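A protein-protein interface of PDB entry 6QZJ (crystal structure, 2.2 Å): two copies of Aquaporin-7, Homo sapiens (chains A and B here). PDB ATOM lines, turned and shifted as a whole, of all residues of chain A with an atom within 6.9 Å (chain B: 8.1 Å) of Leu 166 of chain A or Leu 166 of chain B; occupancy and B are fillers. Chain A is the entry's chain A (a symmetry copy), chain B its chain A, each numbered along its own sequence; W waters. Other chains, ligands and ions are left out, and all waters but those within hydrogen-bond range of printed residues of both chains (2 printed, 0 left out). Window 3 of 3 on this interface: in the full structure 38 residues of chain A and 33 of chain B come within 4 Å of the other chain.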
ATOM      1  N   HIS A  51      10.530 -12.935   9.110  1.00  0.00           N
ATOM      2  CA  HIS A  51       9.523 -13.095  10.151  1.00  0.00           C
ATOM      3  C   HIS A  51       8.329 -13.921   9.680  1.00  0.00           C
ATOM      4  O   HIS A  51       7.665 -14.553  10.509  1.00  0.00           O
ATOM      5  CB  HIS A  51       9.052 -11.730  10.656  1.00  0.00           C
ATOM      6  CG  HIS A  51       9.995 -11.092  11.630  1.00  0.00           C
ATOM      7  ND1 HIS A  51      10.286 -11.651  12.857  1.00  0.00           N
ATOM      8  CD2 HIS A  51      10.727  -9.955  11.549  1.00  0.00           C
ATOM      9  CE1 HIS A  51      11.154 -10.882  13.491  1.00  0.00           C
ATOM     10  NE2 HIS A  51      11.439  -9.848  12.720  1.00  0.00           N
ATOM     11  N   ILE A 157      25.712 -15.241   9.826  1.00  0.00           N
ATOM     12  CA  ILE A 157      24.707 -14.635  10.693  1.00  0.00           C
ATOM     13  C   ILE A 157      23.879 -15.707  11.403  1.00  0.00           C
ATOM     14  O   ILE A 157      23.433 -15.501  12.538  1.00  0.00           O
ATOM     15  CB  ILE A 157      23.814 -13.664   9.894  1.00  0.00           C
ATOM     16  CG1 ILE A 157      24.629 -12.473   9.370  1.00  0.00           C
ATOM     17  CG2 ILE A 157      22.673 -13.150  10.756  1.00  0.00           C
ATOM     18  CD1 ILE A 157      23.895 -11.614   8.331  1.00  0.00           C
ATOM     19  N   GLN A 160      24.916 -21.269  14.314  1.00  0.00           N
ATOM     20  CA  GLN A 160      24.790 -21.435  15.758  1.00  0.00           C
ATOM     21  C   GLN A 160      26.063 -21.953  16.417  1.00  0.00           C
ATOM     22  O   GLN A 160      26.149 -21.936  17.648  1.00  0.00           O
ATOM     23  CB  GLN A 160      23.630 -22.380  16.090  1.00  0.00           C
ATOM     24  CG  GLN A 160      22.272 -21.863  15.665  1.00  0.00           C
ATOM     25  CD  GLN A 160      22.010 -20.458  16.172  1.00  0.00           C
ATOM     26  OE1 GLN A 160      22.154 -20.177  17.363  1.00  0.00           O
ATOM     27  NE2 GLN A 160      21.645 -19.559  15.263  1.00  0.00           N
ATOM     28  N   PRO A 164      26.660 -16.162  15.740  1.00  0.00           N
ATOM     29  CA  PRO A 164      25.425 -15.780  15.063  1.00  0.00           C
ATOM     30  C   PRO A 164      24.735 -14.596  15.738  1.00  0.00           C
ATOM     31  O   PRO A 164      25.026 -14.241  16.881  1.00  0.00           O
ATOM     32  CB  PRO A 164      24.569 -17.043  15.199  1.00  0.00           C
ATOM     33  CG  PRO A 164      24.983 -17.588  16.548  1.00  0.00           C
ATOM     34  CD  PRO A 164      26.440 -17.233  16.733  1.00  0.00           C
ATOM     35  N   ALA A 165      23.795 -14.004  15.005  1.00  0.00           N
ATOM     36  CA  ALA A 165      22.913 -13.006  15.594  1.00  0.00           C
ATOM     37  C   ALA A 165      22.033 -13.658  16.652  1.00  0.00           C
ATOM     38  O   ALA A 165      21.603 -14.802  16.498  1.00  0.00           O
ATOM     39  CB  ALA A 165      22.041 -12.359  14.521  1.00  0.00           C
ATOM     40  N   LEU A 166      21.764 -12.925  17.727  1.00  0.00           N
ATOM     41  CA  LEU A 166      20.961 -13.462  18.819  1.00  0.00           C
ATOM     42  C   LEU A 166      19.596 -13.895  18.290  1.00  0.00           C
ATOM     43  O   LEU A 166      18.966 -13.140  17.529  1.00  0.00           O
ATOM     44  CB  LEU A 166      20.797 -12.416  19.920  1.00  0.00           C
ATOM     45  CG  LEU A 166      20.096 -12.802  21.222  1.00  0.00           C
ATOM     46  CD1 LEU A 166      20.929 -13.755  22.068  1.00  0.00           C
ATOM     47  CD2 LEU A 166      19.793 -11.531  21.983  1.00  0.00           C
ATOM     48  N   PRO A 167      19.123 -15.096  18.638  1.00  0.00           N
ATOM     49  CA  PRO A 167      17.850 -15.580  18.091  1.00  0.00           C
ATOM     50  C   PRO A 167      16.710 -14.625  18.399  1.00  0.00           C
ATOM     51  O   PRO A 167      16.583 -14.113  19.514  1.00  0.00           O
ATOM     52  CB  PRO A 167      17.659 -16.935  18.787  1.00  0.00           C
ATOM     53  CG  PRO A 167      19.051 -17.385  19.110  1.00  0.00           C
ATOM     54  CD  PRO A 167      19.808 -16.122  19.443  1.00  0.00           C
ATOM     55  N   GLY A 168      15.880 -14.380  17.390  1.00  0.00           N
ATOM     56  CA  GLY A 168      14.873 -13.348  17.453  1.00  0.00           C
ATOM     57  C   GLY A 168      15.310 -12.022  16.872  1.00  0.00           C
ATOM     58  O   GLY A 168      14.468 -11.128  16.715  1.00  0.00           O
ATOM     59  N   THR A 169      16.598 -11.863  16.550  1.00  0.00           N
ATOM     60  CA  THR A 169      17.077 -10.671  15.862  1.00  0.00           C
ATOM     61  C   THR A 169      17.734 -10.952  14.515  1.00  0.00           C
ATOM     62  O   THR A 169      18.188 -10.000  13.859  1.00  0.00           O
ATOM     63  CB  THR A 169      18.072  -9.889  16.736  1.00  0.00           C
ATOM     64  OG1 THR A 169      19.366 -10.503  16.657  1.00  0.00           O
ATOM     65  CG2 THR A 169      17.608  -9.832  18.187  1.00  0.00           C
ATOM     66  N   GLU A 170      17.792 -12.213  14.072  1.00  0.00           N
ATOM     67  CA  GLU A 170      18.420 -12.513  12.789  1.00  0.00           C
ATOM     68  C   GLU A 170      17.705 -11.827  11.638  1.00  0.00           C
ATOM     69  O   GLU A 170      18.327 -11.554  10.604  1.00  0.00           O
ATOM     70  CB  GLU A 170      18.455 -14.019  12.539  1.00  0.00           C
ATOM     71  CG  GLU A 170      18.947 -14.802  13.721  1.00  0.00           C
ATOM     72  CD  GLU A 170      17.844 -15.630  14.330  1.00  0.00           C
ATOM     73  OE1 GLU A 170      18.091 -16.816  14.639  1.00  0.00           O
ATOM     74  OE2 GLU A 170      16.726 -15.083  14.472  1.00  0.00           O
ATOM     75  N   ALA A 171      16.404 -11.564  11.784  1.00  0.00           N
ATOM     76  CA  ALA A 171      15.678 -10.854  10.735  1.00  0.00           C
ATOM     77  C   ALA A 171      16.282  -9.475  10.499  1.00  0.00           C
ATOM     78  O   ALA A 171      16.392  -9.026   9.355  1.00  0.00           O
ATOM     79  CB  ALA A 171      14.194 -10.741  11.091  1.00  0.00           C
ATOM     80  N   VAL A 173      19.543  -8.451  11.205  1.00  0.00           N
ATOM     81  CA  VAL A 173      20.900  -8.489  10.678  1.00  0.00           C
ATOM     82  C   VAL A 173      20.899  -8.911   9.213  1.00  0.00           C
ATOM     83  O   VAL A 173      21.700  -8.415   8.412  1.00  0.00           O
ATOM     84  CB  VAL A 173      21.775  -9.409  11.550  1.00  0.00           C
ATOM     85  CG1 VAL A 173      23.233  -9.305  11.145  1.00  0.00           C
ATOM     86  CG2 VAL A 173      21.614  -9.033  13.016  1.00  0.00           C
ATOM     87  N   ILE B 157       5.388 -10.228  13.005  1.00  0.00           N
ATOM     88  CA  ILE B 157       6.411  -9.747  13.927  1.00  0.00           C
ATOM     89  C   ILE B 157       6.069 -10.124  15.368  1.00  0.00           C
ATOM     90  O   ILE B 157       6.969 -10.363  16.182  1.00  0.00           O
ATOM     91  CB  ILE B 157       6.612  -8.225  13.770  1.00  0.00           C
ATOM     92  CG1 ILE B 157       7.167  -7.885  12.380  1.00  0.00           C
ATOM     93  CG2 ILE B 157       7.563  -7.697  14.832  1.00  0.00           C
ATOM     94  CD1 ILE B 157       7.126  -6.390  12.033  1.00  0.00           C
ATOM     95  N   GLN B 160       3.805 -15.194  18.477  1.00  0.00           N
ATOM     96  CA  GLN B 160       4.631 -16.002  19.368  1.00  0.00           C
ATOM     97  C   GLN B 160       4.681 -17.473  18.973  1.00  0.00           C
ATOM     98  O   GLN B 160       5.504 -18.212  19.518  1.00  0.00           O
ATOM     99  CB  GLN B 160       4.134 -15.885  20.813  1.00  0.00           C
ATOM    100  CG  GLN B 160       4.238 -14.488  21.389  1.00  0.00           C
ATOM    101  CD  GLN B 160       5.628 -13.904  21.228  1.00  0.00           C
ATOM    102  OE1 GLN B 160       6.624 -14.529  21.595  1.00  0.00           O
ATOM    103  NE2 GLN B 160       5.704 -12.708  20.653  1.00  0.00           N
ATOM    104  N   ASN B 163       7.534 -16.943  13.974  1.00  0.00           N
ATOM    105  CA  ASN B 163       8.902 -16.427  14.050  1.00  0.00           C
ATOM    106  C   ASN B 163       8.868 -14.951  14.407  1.00  0.00           C
ATOM    107  O   ASN B 163       9.107 -14.073  13.560  1.00  0.00           O
ATOM    108  CB  ASN B 163       9.654 -16.660  12.740  1.00  0.00           C
ATOM    109  CG  ASN B 163      11.128 -16.350  12.861  1.00  0.00           C
ATOM    110  OD1 ASN B 163      11.754 -16.668  13.871  1.00  0.00           O
ATOM    111  ND2 ASN B 163      11.689 -15.706  11.838  1.00  0.00           N
ATOM    112  N   PRO B 164       8.595 -14.628  15.666  1.00  0.00           N
ATOM    113  CA  PRO B 164       8.431 -13.239  16.082  1.00  0.00           C
ATOM    114  C   PRO B 164       9.763 -12.575  16.421  1.00  0.00           C
ATOM    115  O   PRO B 164      10.785 -13.233  16.622  1.00  0.00           O
ATOM    116  CB  PRO B 164       7.567 -13.372  17.340  1.00  0.00           C
ATOM    117  CG  PRO B 164       8.047 -14.672  17.945  1.00  0.00           C
ATOM    118  CD  PRO B 164       8.441 -15.568  16.795  1.00  0.00           C
ATOM    119  N   ALA B 165       9.723 -11.246  16.497  1.00  0.00           N
ATOM    120  CA  ALA B 165      10.858 -10.498  17.018  1.00  0.00           C
ATOM    121  C   ALA B 165      11.061 -10.828  18.491  1.00  0.00           C
ATOM    122  O   ALA B 165      10.097 -11.021  19.233  1.00  0.00           O
ATOM    123  CB  ALA B 165      10.634  -8.997  16.849  1.00  0.00           C
ATOM    124  N   LEU B 166      12.320 -10.889  18.912  1.00  0.00           N
ATOM    125  CA  LEU B 166      12.631 -11.234  20.294  1.00  0.00           C
ATOM    126  C   LEU B 166      11.952 -10.244  21.237  1.00  0.00           C
ATOM    127  O   LEU B 166      12.016  -9.026  20.998  1.00  0.00           O
ATOM    128  CB  LEU B 166      14.143 -11.225  20.514  1.00  0.00           C
ATOM    129  CG  LEU B 166      14.707 -11.680  21.859  1.00  0.00           C
ATOM    130  CD1 LEU B 166      14.551 -13.179  22.076  1.00  0.00           C
ATOM    131  CD2 LEU B 166      16.163 -11.277  21.914  1.00  0.00           C
ATOM    132  N   PRO B 167      11.275 -10.718  22.288  1.00  0.00           N
ATOM    133  CA  PRO B 167      10.546  -9.806  23.176  1.00  0.00           C
ATOM    134  C   PRO B 167      11.464  -8.749  23.767  1.00  0.00           C
ATOM    135  O   PRO B 167      12.582  -9.036  24.198  1.00  0.00           O
ATOM    136  CB  PRO B 167       9.984 -10.738  24.257  1.00  0.00           C
ATOM    137  CG  PRO B 167       9.864 -12.066  23.575  1.00  0.00           C
ATOM    138  CD  PRO B 167      11.037 -12.132  22.627  1.00  0.00           C
ATOM    139  N   GLY B 168      10.979  -7.510  23.774  1.00  0.00           N
ATOM    140  CA  GLY B 168      11.794  -6.367  24.108  1.00  0.00           C
ATOM    141  C   GLY B 168      12.411  -5.676  22.913  1.00  0.00           C
ATOM    142  O   GLY B 168      12.976  -4.587  23.074  1.00  0.00           O
ATOM    143  N   THR B 169      12.323  -6.273  21.719  1.00  0.00           N
ATOM    144  CA  THR B 169      12.769  -5.616  20.497  1.00  0.00           C
ATOM    145  C   THR B 169      11.673  -5.436  19.453  1.00  0.00           C
ATOM    146  O   THR B 169      11.958  -4.900  18.370  1.00  0.00           O
ATOM    147  CB  THR B 169      13.937  -6.381  19.852  1.00  0.00           C
ATOM    148  OG1 THR B 169      13.428  -7.500  19.113  1.00  0.00           O
ATOM    149  CG2 THR B 169      14.933  -6.857  20.902  1.00  0.00           C
ATOM    150  N   GLU B 170      10.433  -5.850  19.736  1.00  0.00           N
ATOM    151  CA  GLU B 170       9.364  -5.696  18.754  1.00  0.00           C
ATOM    152  C   GLU B 170       9.119  -4.237  18.411  1.00  0.00           C
ATOM    153  O   GLU B 170       8.646  -3.935  17.309  1.00  0.00           O
ATOM    154  CB  GLU B 170       8.066  -6.323  19.257  1.00  0.00           C
ATOM    155  CG  GLU B 170       8.257  -7.699  19.824  1.00  0.00           C
ATOM    156  CD  GLU B 170       8.031  -7.717  21.315  1.00  0.00           C
ATOM    157  OE1 GLU B 170       7.344  -8.641  21.801  1.00  0.00           O
ATOM    158  OE2 GLU B 170       8.531  -6.784  21.983  1.00  0.00           O
ATOM    159  N   ALA B 171       9.408  -3.324  19.343  1.00  0.00           N
ATOM    160  CA  ALA B 171       9.249  -1.903  19.049  1.00  0.00           C
ATOM    161  C   ALA B 171      10.133  -1.490  17.879  1.00  0.00           C
ATOM    162  O   ALA B 171       9.718  -0.700  17.027  1.00  0.00           O
ATOM    163  CB  ALA B 171       9.563  -1.061  20.288  1.00  0.00           C
ATOM    164  N   LEU B 172      11.350  -2.039  17.817  1.00  0.00           N
ATOM    165  CA  LEU B 172      12.271  -1.739  16.723  1.00  0.00           C
ATOM    166  C   LEU B 172      11.735  -2.261  15.397  1.00  0.00           C
ATOM    167  O   LEU B 172      11.627  -1.513  14.419  1.00  0.00           O
ATOM    168  CB  LEU B 172      13.640  -2.352  17.021  1.00  0.00           C
ATOM    169  CG  LEU B 172      14.892  -1.552  16.674  1.00  0.00           C
ATOM    170  CD1 LEU B 172      15.045  -0.405  17.655  1.00  0.00           C
ATOM    171  CD2 LEU B 172      16.136  -2.446  16.685  1.00  0.00           C
ATOM    172  N   VAL B 173      11.382  -3.546  15.351  1.00  0.00           N
ATOM    173  CA  VAL B 173      11.011  -4.172  14.088  1.00  0.00           C
ATOM    174  C   VAL B 173       9.729  -3.558  13.538  1.00  0.00           C
ATOM    175  O   VAL B 173       9.578  -3.396  12.321  1.00  0.00           O
ATOM    176  CB  VAL B 173      10.896  -5.697  14.272  1.00  0.00           C
ATOM    177  CG1 VAL B 173      10.714  -6.387  12.935  1.00  0.00           C
ATOM    178  CG2 VAL B 173      12.144  -6.226  14.965  1.00  0.00           C
HETATM  179  O   HOH W   1       6.290 -14.779  12.622  1.00  0.00           O
HETATM  180  O   HOH W   2      14.291  -8.568  16.548  1.00  0.00           O
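The backbone carbonyl oxygen (O) of Asn 163 of chain B lies within hydrogen-bond range of a ring nitrogen (ND1) of His 51 of chain A, at 2.8 Å. N of Leu 166 of chain B lies within hydrogen-bond range of O of Gly 168 of chain A, at 3.1 Å.
Printed residues of chain A that touch a printed residue of chain B: His 51, Leu 166, Pro 167 and Gly 168. Hydrophobic or aromatic side chains of chain A that line the printed part of chain B: His 51 and Leu 166. Of the 13 printed residues of chain B, 5 touch a printed residue of chain A. Along chain B the printed residues that touch a printed residue of chain A span positions 163 to 173. Among the printed residues, no Asp or Glu carboxylate lies within 4 Å of a Lys or Arg side-chain nitrogen of the other chain.
Printed residues of chain B within 4 Å of His 51 of chain A: Asn 163, Pro 164, Ala 165 and Val 173. No residue of chain B comes within 4 Å of Ala 165 of chain A. Leu 166 of chain A touches just one residue of chain B: Leu 166. Gly 168 of chain A touches just these residues of chain B: Ala 165 and Leu 166. Of the printed residues of chain A, Pro 164 of chain B touches His 51. Of the printed residues of chain A, Val 173 of chain B touches His 51 (3.5 Å). The nearest residue of chain B that does not touch Leu 166 of chain A is Thr 169 of chain B (6.8 Å). The nearest residue of chain A that does not touch Leu 166 of chain B is Thr 169 of chain A (4.3 Å). The nearest printed residue of chain B that does not touch His 51 of chain A is Ile 157 of chain B (4.2 Å).
Water W1 lies within hydrogen-bond range of O of His 51 of chain A (2.5 Å) and N of Asn 163 of chain B (2.8 Å). Water W2 bridges O of Gly 168 of chain A (2.6 Å) and OG1 of Thr 169 of chain B (2.9 Å).
Among the printed residues, merely in contact across the chains: His 51 of chain A with Ala 165 of chain B (3.3 Å), Pro 167 of chain A with Leu 166 of chain B (3.4 Å), His 51 of chain A with Val 173 of chain B (3.5 Å), Leu 166 of chain A with Leu 166 of chain B (3.6 Å), His 51 of chain A with Pro 164 of chain B (3.7 Å) and Gly 168 of chain A with Ala 165 of chain B (3.7 Å).
The backbone carbonyl oxygen (O) of Leu 166 of chain A sits at hydrogen-bond distance from the side-chain hydroxyl (OG1) of Thr 169 of chain A. The backbone carbonyl oxygen (O) of Leu 166 of chain B lies within hydrogen-bond range of the side-chain hydroxyl (OG1) of Thr 169 of chain B, at 2.8 Å. The backbone NH (N) of Ala 165 of chain B is in hydrogen-bond range of the backbone carbonyl oxygen (O) of Ile 157 of chain B, 2.9 Å away. The backbone NH (N) of Gly 168 of chain A lies within hydrogen-bond range of the side-chain carboxylate (OE2) of Glu 170 of chain A (3.1 Å).
Leu 166 of chain A touches its own counterpart, Leu 166 of chain B. Pro 167 of chain A touches Leu 166 of chain B, but with the chains exchanged Leu 166 of chain A does not touch Pro 167 of chain B (7.9 Å). Gly 168 of chain A touches Ala 165 of chain B, but with the chains exchanged Ala 165 of chain A does not touch Gly 168 of chain B (14.0 Å). Gly 168 of chain A touches Leu 166 of chain B, but with the chains exchanged Leu 166 of chain A does not touch Gly 168 of chain B (9.5 Å). Of the 8 pairs that touch across the chains among the printed residues, 1 has its exchanged pair printed and touching as well.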
